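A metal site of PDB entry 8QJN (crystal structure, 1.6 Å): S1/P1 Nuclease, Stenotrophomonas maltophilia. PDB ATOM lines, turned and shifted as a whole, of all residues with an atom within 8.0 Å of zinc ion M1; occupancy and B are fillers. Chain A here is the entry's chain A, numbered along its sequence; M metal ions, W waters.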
ATOM      1  N   TRP A   1     -31.109   2.716  13.709  1.00  0.00           N
ATOM      2  CA  TRP A   1     -31.118   4.166  13.478  1.00  0.00           C
ATOM      3  C   TRP A   1     -30.067   4.841  14.361  1.00  0.00           C
ATOM      4  O   TRP A   1     -29.684   4.243  15.416  1.00  0.00           O
ATOM      5  CB  TRP A   1     -32.519   4.786  13.759  1.00  0.00           C
ATOM      6  CG  TRP A   1     -33.621   4.131  12.991  1.00  0.00           C
ATOM      7  CD1 TRP A   1     -34.524   3.228  13.493  1.00  0.00           C
ATOM      8  CD2 TRP A   1     -33.964   4.319  11.605  1.00  0.00           C
ATOM      9  NE1 TRP A   1     -35.373   2.819  12.498  1.00  0.00           N
ATOM     10  CE2 TRP A   1     -35.087   3.507  11.338  1.00  0.00           C
ATOM     11  CE3 TRP A   1     -33.481   5.151  10.582  1.00  0.00           C
ATOM     12  CZ2 TRP A   1     -35.702   3.473  10.089  1.00  0.00           C
ATOM     13  CZ3 TRP A   1     -34.061   5.081   9.328  1.00  0.00           C
ATOM     14  CH2 TRP A   1     -35.155   4.249   9.072  1.00  0.00           C
ATOM     15  N   GLY A   2     -29.689   6.049  13.986  1.00  0.00           N
ATOM     16  CA  GLY A   2     -29.036   7.006  14.900  1.00  0.00           C
ATOM     17  C   GLY A   2     -30.023   7.578  15.878  1.00  0.00           C
ATOM     18  O   GLY A   2     -31.213   7.177  15.832  1.00  0.00           O
ATOM     19  N   HIS A   6     -34.360   7.110  16.319  1.00  0.00           N
ATOM     20  CA  HIS A   6     -34.956   6.488  17.523  1.00  0.00           C
ATOM     21  C   HIS A   6     -35.916   7.440  18.202  1.00  0.00           C
ATOM     22  O   HIS A   6     -37.042   6.967  18.553  1.00  0.00           O
ATOM     23  CB  HIS A   6     -33.890   5.977  18.480  1.00  0.00           C
ATOM     24  CG  HIS A   6     -33.310   4.728  17.923  1.00  0.00           C
ATOM     25  ND1 HIS A   6     -34.027   3.557  17.866  1.00  0.00           N
ATOM     26  CD2 HIS A   6     -32.117   4.487  17.359  1.00  0.00           C
ATOM     27  CE1 HIS A   6     -33.268   2.627  17.311  1.00  0.00           C
ATOM     28  NE2 HIS A   6     -32.081   3.169  16.971  1.00  0.00           N
ATOM     29  N   ASP A  45     -28.339   2.246  22.695  1.00  0.00           N
ATOM     30  CA  ASP A  45     -27.094   2.488  21.922  1.00  0.00           C
ATOM     31  C   ASP A  45     -26.003   3.054  22.837  1.00  0.00           C
ATOM     32  O   ASP A  45     -24.837   2.827  22.539  1.00  0.00           O
ATOM     33  CB  ASP A  45     -27.322   3.412  20.717  1.00  0.00           C
ATOM     34  CG  ASP A  45     -27.996   2.735  19.516  1.00  0.00           C
ATOM     35  OD1 ASP A  45     -28.094   1.494  19.494  1.00  0.00           O
ATOM     36  OD2 ASP A  45     -28.459   3.476  18.593  1.00  0.00           O
ATOM     37  N   ARG A  48     -24.755   0.009  25.158  1.00  0.00           N
ATOM     38  CA  ARG A  48     -23.867  -0.800  24.284  1.00  0.00           C
ATOM     39  C   ARG A  48     -22.519  -0.092  24.106  1.00  0.00           C
ATOM     40  O   ARG A  48     -21.472  -0.788  24.022  1.00  0.00           O
ATOM     41  CB  ARG A  48     -24.519  -1.018  22.922  1.00  0.00           C
ATOM     42  CG  ARG A  48     -23.714  -1.901  21.988  1.00  0.00           C
ATOM     43  CD  ARG A  48     -24.252  -1.846  20.568  1.00  0.00           C
ATOM     44  NE  ARG A  48     -24.232  -0.485  20.051  1.00  0.00           N
ATOM     45  CZ  ARG A  48     -25.084   0.003  19.147  1.00  0.00           C
ATOM     46  NH1 ARG A  48     -26.032  -0.761  18.644  1.00  0.00           N
ATOM     47  NH2 ARG A  48     -24.983   1.265  18.761  1.00  0.00           N
ATOM     48  N   HIS A  62     -29.542  -5.584  18.598  1.00  0.00           N
ATOM     49  CA  HIS A  62     -29.947  -4.464  17.724  1.00  0.00           C
ATOM     50  C   HIS A  62     -30.231  -4.943  16.295  1.00  0.00           C
ATOM     51  O   HIS A  62     -30.693  -4.139  15.493  1.00  0.00           O
ATOM     52  CB  HIS A  62     -28.929  -3.348  17.771  1.00  0.00           C
ATOM     53  CG  HIS A  62     -28.811  -2.717  19.096  1.00  0.00           C
ATOM     54  ND1 HIS A  62     -29.051  -1.370  19.306  1.00  0.00           N
ATOM     55  CD2 HIS A  62     -28.415  -3.247  20.276  1.00  0.00           C
ATOM     56  CE1 HIS A  62     -28.869  -1.122  20.587  1.00  0.00           C
ATOM     57  NE2 HIS A  62     -28.485  -2.252  21.212  1.00  0.00           N
ATOM     58  N   TYR A  63     -29.915  -6.167  15.943  1.00  0.00           N
ATOM     59  CA  TYR A  63     -30.017  -6.585  14.520  1.00  0.00           C
ATOM     60  C   TYR A  63     -30.262  -8.077  14.389  1.00  0.00           C
ATOM     61  O   TYR A  63     -30.278  -8.835  15.368  1.00  0.00           O
ATOM     62  CB  TYR A  63     -28.759  -6.153  13.759  1.00  0.00           C
ATOM     63  CG  TYR A  63     -27.491  -6.648  14.357  1.00  0.00           C
ATOM     64  CD1 TYR A  63     -27.010  -7.918  14.040  1.00  0.00           C
ATOM     65  CD2 TYR A  63     -26.779  -5.887  15.272  1.00  0.00           C
ATOM     66  CE1 TYR A  63     -25.842  -8.410  14.614  1.00  0.00           C
ATOM     67  CE2 TYR A  63     -25.619  -6.367  15.854  1.00  0.00           C
ATOM     68  CZ  TYR A  63     -25.156  -7.625  15.526  1.00  0.00           C
ATOM     69  OH  TYR A  63     -23.993  -8.113  16.088  1.00  0.00           O
ATOM     70  N   HIS A 115     -36.518   1.173  21.697  1.00  0.00           N
ATOM     71  CA  HIS A 115     -35.317   1.220  20.842  1.00  0.00           C
ATOM     72  C   HIS A 115     -35.478   0.119  19.775  1.00  0.00           C
ATOM     73  O   HIS A 115     -35.248   0.405  18.590  1.00  0.00           O
ATOM     74  CB  HIS A 115     -34.034   1.001  21.656  1.00  0.00           C
ATOM     75  CG  HIS A 115     -32.810   1.225  20.829  1.00  0.00           C
ATOM     76  ND1 HIS A 115     -32.221   2.465  20.717  1.00  0.00           N
ATOM     77  CD2 HIS A 115     -32.085   0.394  20.052  1.00  0.00           C
ATOM     78  CE1 HIS A 115     -31.169   2.392  19.935  1.00  0.00           C
ATOM     79  NE2 HIS A 115     -31.056   1.144  19.492  1.00  0.00           N
ATOM     80  N   ASP A 119     -35.169  -0.198  15.681  1.00  0.00           N
ATOM     81  CA  ASP A 119     -34.054  -0.856  14.965  1.00  0.00           C
ATOM     82  C   ASP A 119     -34.610  -1.950  14.054  1.00  0.00           C
ATOM     83  O   ASP A 119     -34.056  -2.143  12.935  1.00  0.00           O
ATOM     84  CB  ASP A 119     -32.977  -1.400  15.888  1.00  0.00           C
ATOM     85  CG  ASP A 119     -31.877  -0.431  16.223  1.00  0.00           C
ATOM     86  OD1 ASP A 119     -31.873   0.649  15.614  1.00  0.00           O
ATOM     87  OD2 ASP A 119     -30.986  -0.779  17.109  1.00  0.00           O
ATOM     88  N   GLN A 122     -35.299  -0.652  10.653  1.00  0.00           N
ATOM     89  CA  GLN A 122     -34.160  -0.115   9.855  1.00  0.00           C
ATOM     90  C   GLN A 122     -33.673  -1.247   8.947  1.00  0.00           C
ATOM     91  O   GLN A 122     -33.142  -2.246   9.422  1.00  0.00           O
ATOM     92  CB  GLN A 122     -33.031   0.407  10.744  1.00  0.00           C
ATOM     93  CG  GLN A 122     -32.234   1.569  10.131  1.00  0.00           C
ATOM     94  CD  GLN A 122     -31.283   1.183   9.029  1.00  0.00           C
ATOM     95  OE1 GLN A 122     -31.673   0.666   7.994  1.00  0.00           O
ATOM     96  NE2 GLN A 122     -30.001   1.485   9.227  1.00  0.00           N
ATOM     97  N   MET A 124     -31.221  -1.991   7.147  1.00  0.00           N
ATOM     98  CA  MET A 124     -29.807  -2.423   7.274  1.00  0.00           C
ATOM     99  C   MET A 124     -29.584  -3.163   8.597  1.00  0.00           C
ATOM    100  O   MET A 124     -28.599  -3.910   8.706  1.00  0.00           O
ATOM    101  CB  MET A 124     -28.838  -1.249   7.176  1.00  0.00           C
ATOM    102  CG  MET A 124     -28.789  -0.660   5.799  1.00  0.00           C
ATOM    103  SD  MET A 124     -28.158  -1.818   4.588  1.00  0.00           S
ATOM    104  CE  MET A 124     -29.401  -1.572   3.326  1.00  0.00           C
ATOM    105  N   HIS A 125     -30.527  -3.071   9.531  1.00  0.00           N
ATOM    106  CA  HIS A 125     -30.462  -3.871  10.777  1.00  0.00           C
ATOM    107  C   HIS A 125     -31.032  -5.288  10.535  1.00  0.00           C
ATOM    108  O   HIS A 125     -31.054  -6.055  11.496  1.00  0.00           O
ATOM    109  CB  HIS A 125     -31.178  -3.144  11.917  1.00  0.00           C
ATOM    110  CG  HIS A 125     -30.378  -2.077  12.550  1.00  0.00           C
ATOM    111  ND1 HIS A 125     -30.033  -2.127  13.860  1.00  0.00           N
ATOM    112  CD2 HIS A 125     -29.755  -0.981  12.048  1.00  0.00           C
ATOM    113  CE1 HIS A 125     -29.255  -1.108  14.156  1.00  0.00           C
ATOM    114  NE2 HIS A 125     -29.103  -0.357  13.084  1.00  0.00           N
ATOM    115  N   LYS A 132     -21.808  -7.022   7.628  1.00  0.00           N
ATOM    116  CA  LYS A 132     -22.269  -6.388   8.891  1.00  0.00           C
ATOM    117  C   LYS A 132     -23.372  -5.372   8.596  1.00  0.00           C
ATOM    118  O   LYS A 132     -23.255  -4.195   9.016  1.00  0.00           O
ATOM    119  CB  LYS A 132     -21.101  -5.761   9.650  1.00  0.00           C
ATOM    120  CG  LYS A 132     -20.069  -6.754  10.162  1.00  0.00           C
ATOM    121  CD  LYS A 132     -18.894  -6.046  10.838  1.00  0.00           C
ATOM    122  CE  LYS A 132     -17.973  -7.024  11.551  1.00  0.00           C
ATOM    123  NZ  LYS A 132     -17.455  -8.052  10.623  1.00  0.00           N
ATOM    124  N   GLY A 133     -24.448  -5.794   7.957  1.00  0.00           N
ATOM    125  CA  GLY A 133     -25.606  -4.916   7.672  1.00  0.00           C
ATOM    126  C   GLY A 133     -25.194  -3.677   6.861  1.00  0.00           C
ATOM    127  O   GLY A 133     -25.688  -2.596   7.117  1.00  0.00           O
ATOM    128  N   ASN A 135     -22.282  -2.134   6.859  1.00  0.00           N
ATOM    129  CA  ASN A 135     -21.214  -1.344   7.517  1.00  0.00           C
ATOM    130  C   ASN A 135     -19.921  -1.418   6.682  1.00  0.00           C
ATOM    131  O   ASN A 135     -19.228  -0.412   6.610  1.00  0.00           O
ATOM    132  CB  ASN A 135     -20.889  -1.824   8.924  1.00  0.00           C
ATOM    133  CG  ASN A 135     -21.689  -1.093   9.974  1.00  0.00           C
ATOM    134  OD1 ASN A 135     -21.543   0.125  10.122  1.00  0.00           O
ATOM    135  ND2 ASN A 135     -22.540  -1.846  10.662  1.00  0.00           N
ATOM    136  N   ASN A 147     -20.705   4.941   4.861  1.00  0.00           N
ATOM    137  CA  ASN A 147     -20.967   3.521   4.566  1.00  0.00           C
ATOM    138  C   ASN A 147     -22.497   3.326   4.487  1.00  0.00           C
ATOM    139  O   ASN A 147     -23.230   4.211   4.914  1.00  0.00           O
ATOM    140  CB  ASN A 147     -20.275   2.609   5.580  1.00  0.00           C
ATOM    141  CG  ASN A 147     -20.926   2.655   6.933  1.00  0.00           C
ATOM    142  OD1 ASN A 147     -22.040   2.166   7.157  1.00  0.00           O
ATOM    143  ND2 ASN A 147     -20.241   3.268   7.866  1.00  0.00           N
ATOM    144  N   HIS A 149     -24.663   1.294   5.876  1.00  0.00           N
ATOM    145  CA  HIS A 149     -25.310   1.215   7.200  1.00  0.00           C
ATOM    146  C   HIS A 149     -25.586   2.611   7.767  1.00  0.00           C
ATOM    147  O   HIS A 149     -26.790   2.881   8.140  1.00  0.00           O
ATOM    148  CB  HIS A 149     -24.529   0.364   8.183  1.00  0.00           C
ATOM    149  CG  HIS A 149     -25.362   0.080   9.376  1.00  0.00           C
ATOM    150  ND1 HIS A 149     -26.032  -1.101   9.499  1.00  0.00           N
ATOM    151  CD2 HIS A 149     -25.652   0.804  10.480  1.00  0.00           C
ATOM    152  CE1 HIS A 149     -26.726  -1.087  10.622  1.00  0.00           C
ATOM    153  NE2 HIS A 149     -26.488   0.044  11.273  1.00  0.00           N
ATOM    154  N   SER A 150     -24.565   3.456   7.840  1.00  0.00           N
ATOM    155  CA  SER A 150     -24.672   4.827   8.382  1.00  0.00           C
ATOM    156  C   SER A 150     -25.583   5.655   7.495  1.00  0.00           C
ATOM    157  O   SER A 150     -26.280   6.539   8.029  1.00  0.00           O
ATOM    158  CB  SER A 150     -23.349   5.510   8.513  1.00  0.00           C
ATOM    159  OG  SER A 150     -22.603   4.879   9.535  1.00  0.00           O
ATOM    160  N   TRP A 152     -28.270   4.758   5.988  1.00  0.00           N
ATOM    161  CA  TRP A 152     -29.662   4.420   6.352  1.00  0.00           C
ATOM    162  C   TRP A 152     -29.932   4.780   7.813  1.00  0.00           C
ATOM    163  O   TRP A 152     -31.050   5.267   8.073  1.00  0.00           O
ATOM    164  CB  TRP A 152     -29.969   2.956   6.039  1.00  0.00           C
ATOM    165  CG  TRP A 152     -30.279   2.803   4.598  1.00  0.00           C
ATOM    166  CD1 TRP A 152     -29.386   2.678   3.569  1.00  0.00           C
ATOM    167  CD2 TRP A 152     -31.579   2.804   4.004  1.00  0.00           C
ATOM    168  NE1 TRP A 152     -30.038   2.597   2.371  1.00  0.00           N
ATOM    169  CE2 TRP A 152     -31.391   2.680   2.602  1.00  0.00           C
ATOM    170  CE3 TRP A 152     -32.879   2.932   4.490  1.00  0.00           C
ATOM    171  CZ2 TRP A 152     -32.454   2.602   1.723  1.00  0.00           C
ATOM    172  CZ3 TRP A 152     -33.930   2.860   3.615  1.00  0.00           C
ATOM    173  CH2 TRP A 152     -33.721   2.700   2.248  1.00  0.00           C
ATOM    174  N   ASP A 153     -28.983   4.614   8.711  1.00  0.00           N
ATOM    175  CA  ASP A 153     -29.199   5.009  10.132  1.00  0.00           C
ATOM    176  C   ASP A 153     -29.409   6.525  10.263  1.00  0.00           C
ATOM    177  O   ASP A 153     -30.264   6.890  11.053  1.00  0.00           O
ATOM    178  CB  ASP A 153     -28.062   4.598  11.056  1.00  0.00           C
ATOM    179  CG  ASP A 153     -28.127   3.215  11.637  1.00  0.00           C
ATOM    180  OD1 ASP A 153     -29.103   2.501  11.382  1.00  0.00           O
ATOM    181  OD2 ASP A 153     -27.202   2.886  12.381  1.00  0.00           O
ATOM    182  N   SER A 154     -28.661   7.379   9.547  1.00  0.00           N
ATOM    183  CA  SER A 154     -28.691   8.829   9.815  1.00  0.00           C
ATOM    184  C   SER A 154     -28.339   9.663   8.599  1.00  0.00           C
ATOM    185  O   SER A 154     -28.792  10.792   8.562  1.00  0.00           O
ATOM    186  CB  SER A 154     -27.781   9.144  10.969  1.00  0.00           C
ATOM    187  OG  SER A 154     -26.435   8.858  10.611  1.00  0.00           O
HETATM  188 ZN    ZN M   1     -27.458   0.896  12.847  1.00  0.00          ZN
HETATM  189 ZN    ZN M   2     -30.671   2.321  15.794  1.00  0.00          ZN
HETATM  190 ZN    ZN M   3     -29.669   0.224  18.243  1.00  0.00          ZN
HETATM  191  O   HOH W   1     -28.351   2.083  14.917  1.00  0.00           O
HETATM  192  O   HOH W   2     -26.291   0.772  14.670  1.00  0.00           O
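Within 4 Å of zinc ion M1: His 125, His 149 and Asp 153.
OD1 of Asp 153 sits at hydrogen-bond distance from NE2 of Gln 122 (2.5 Å).
ND1 of His 149 is in hydrogen-bond range of O of Gly 133, 2.8 Å away.
A ring nitrogen (ND1) of His 125 sits at hydrogen-bond distance from the backbone carbonyl oxygen of His 62 (2.7 Å).
The side-chain carboxylate of Asp 153 sits close to the backbone NH of Trp 1, at 3.1 Å.
The backbone NH (N) of Gly 2 lies within hydrogen-bond range of the backbone carbonyl oxygen (O) of Asp 153 (3.1 Å).
The side-chain amide oxygen (OD1) of Asn 147 sits at hydrogen-bond distance from the backbone NH (N) of His 149 (3.0 Å).
Zinc ion M1 is bound by NE2 of His 149 (2.0 Å), OD2 of Asp 153 (2.1 Å), NE2 of His 125 (2.1 Å), water W2 (2.2 Å) and water W1 (2.5 Å).
Slightly farther from zinc ion M1 lies the side-chain carboxylate (OD1) of Asp 153 (2.7 Å).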
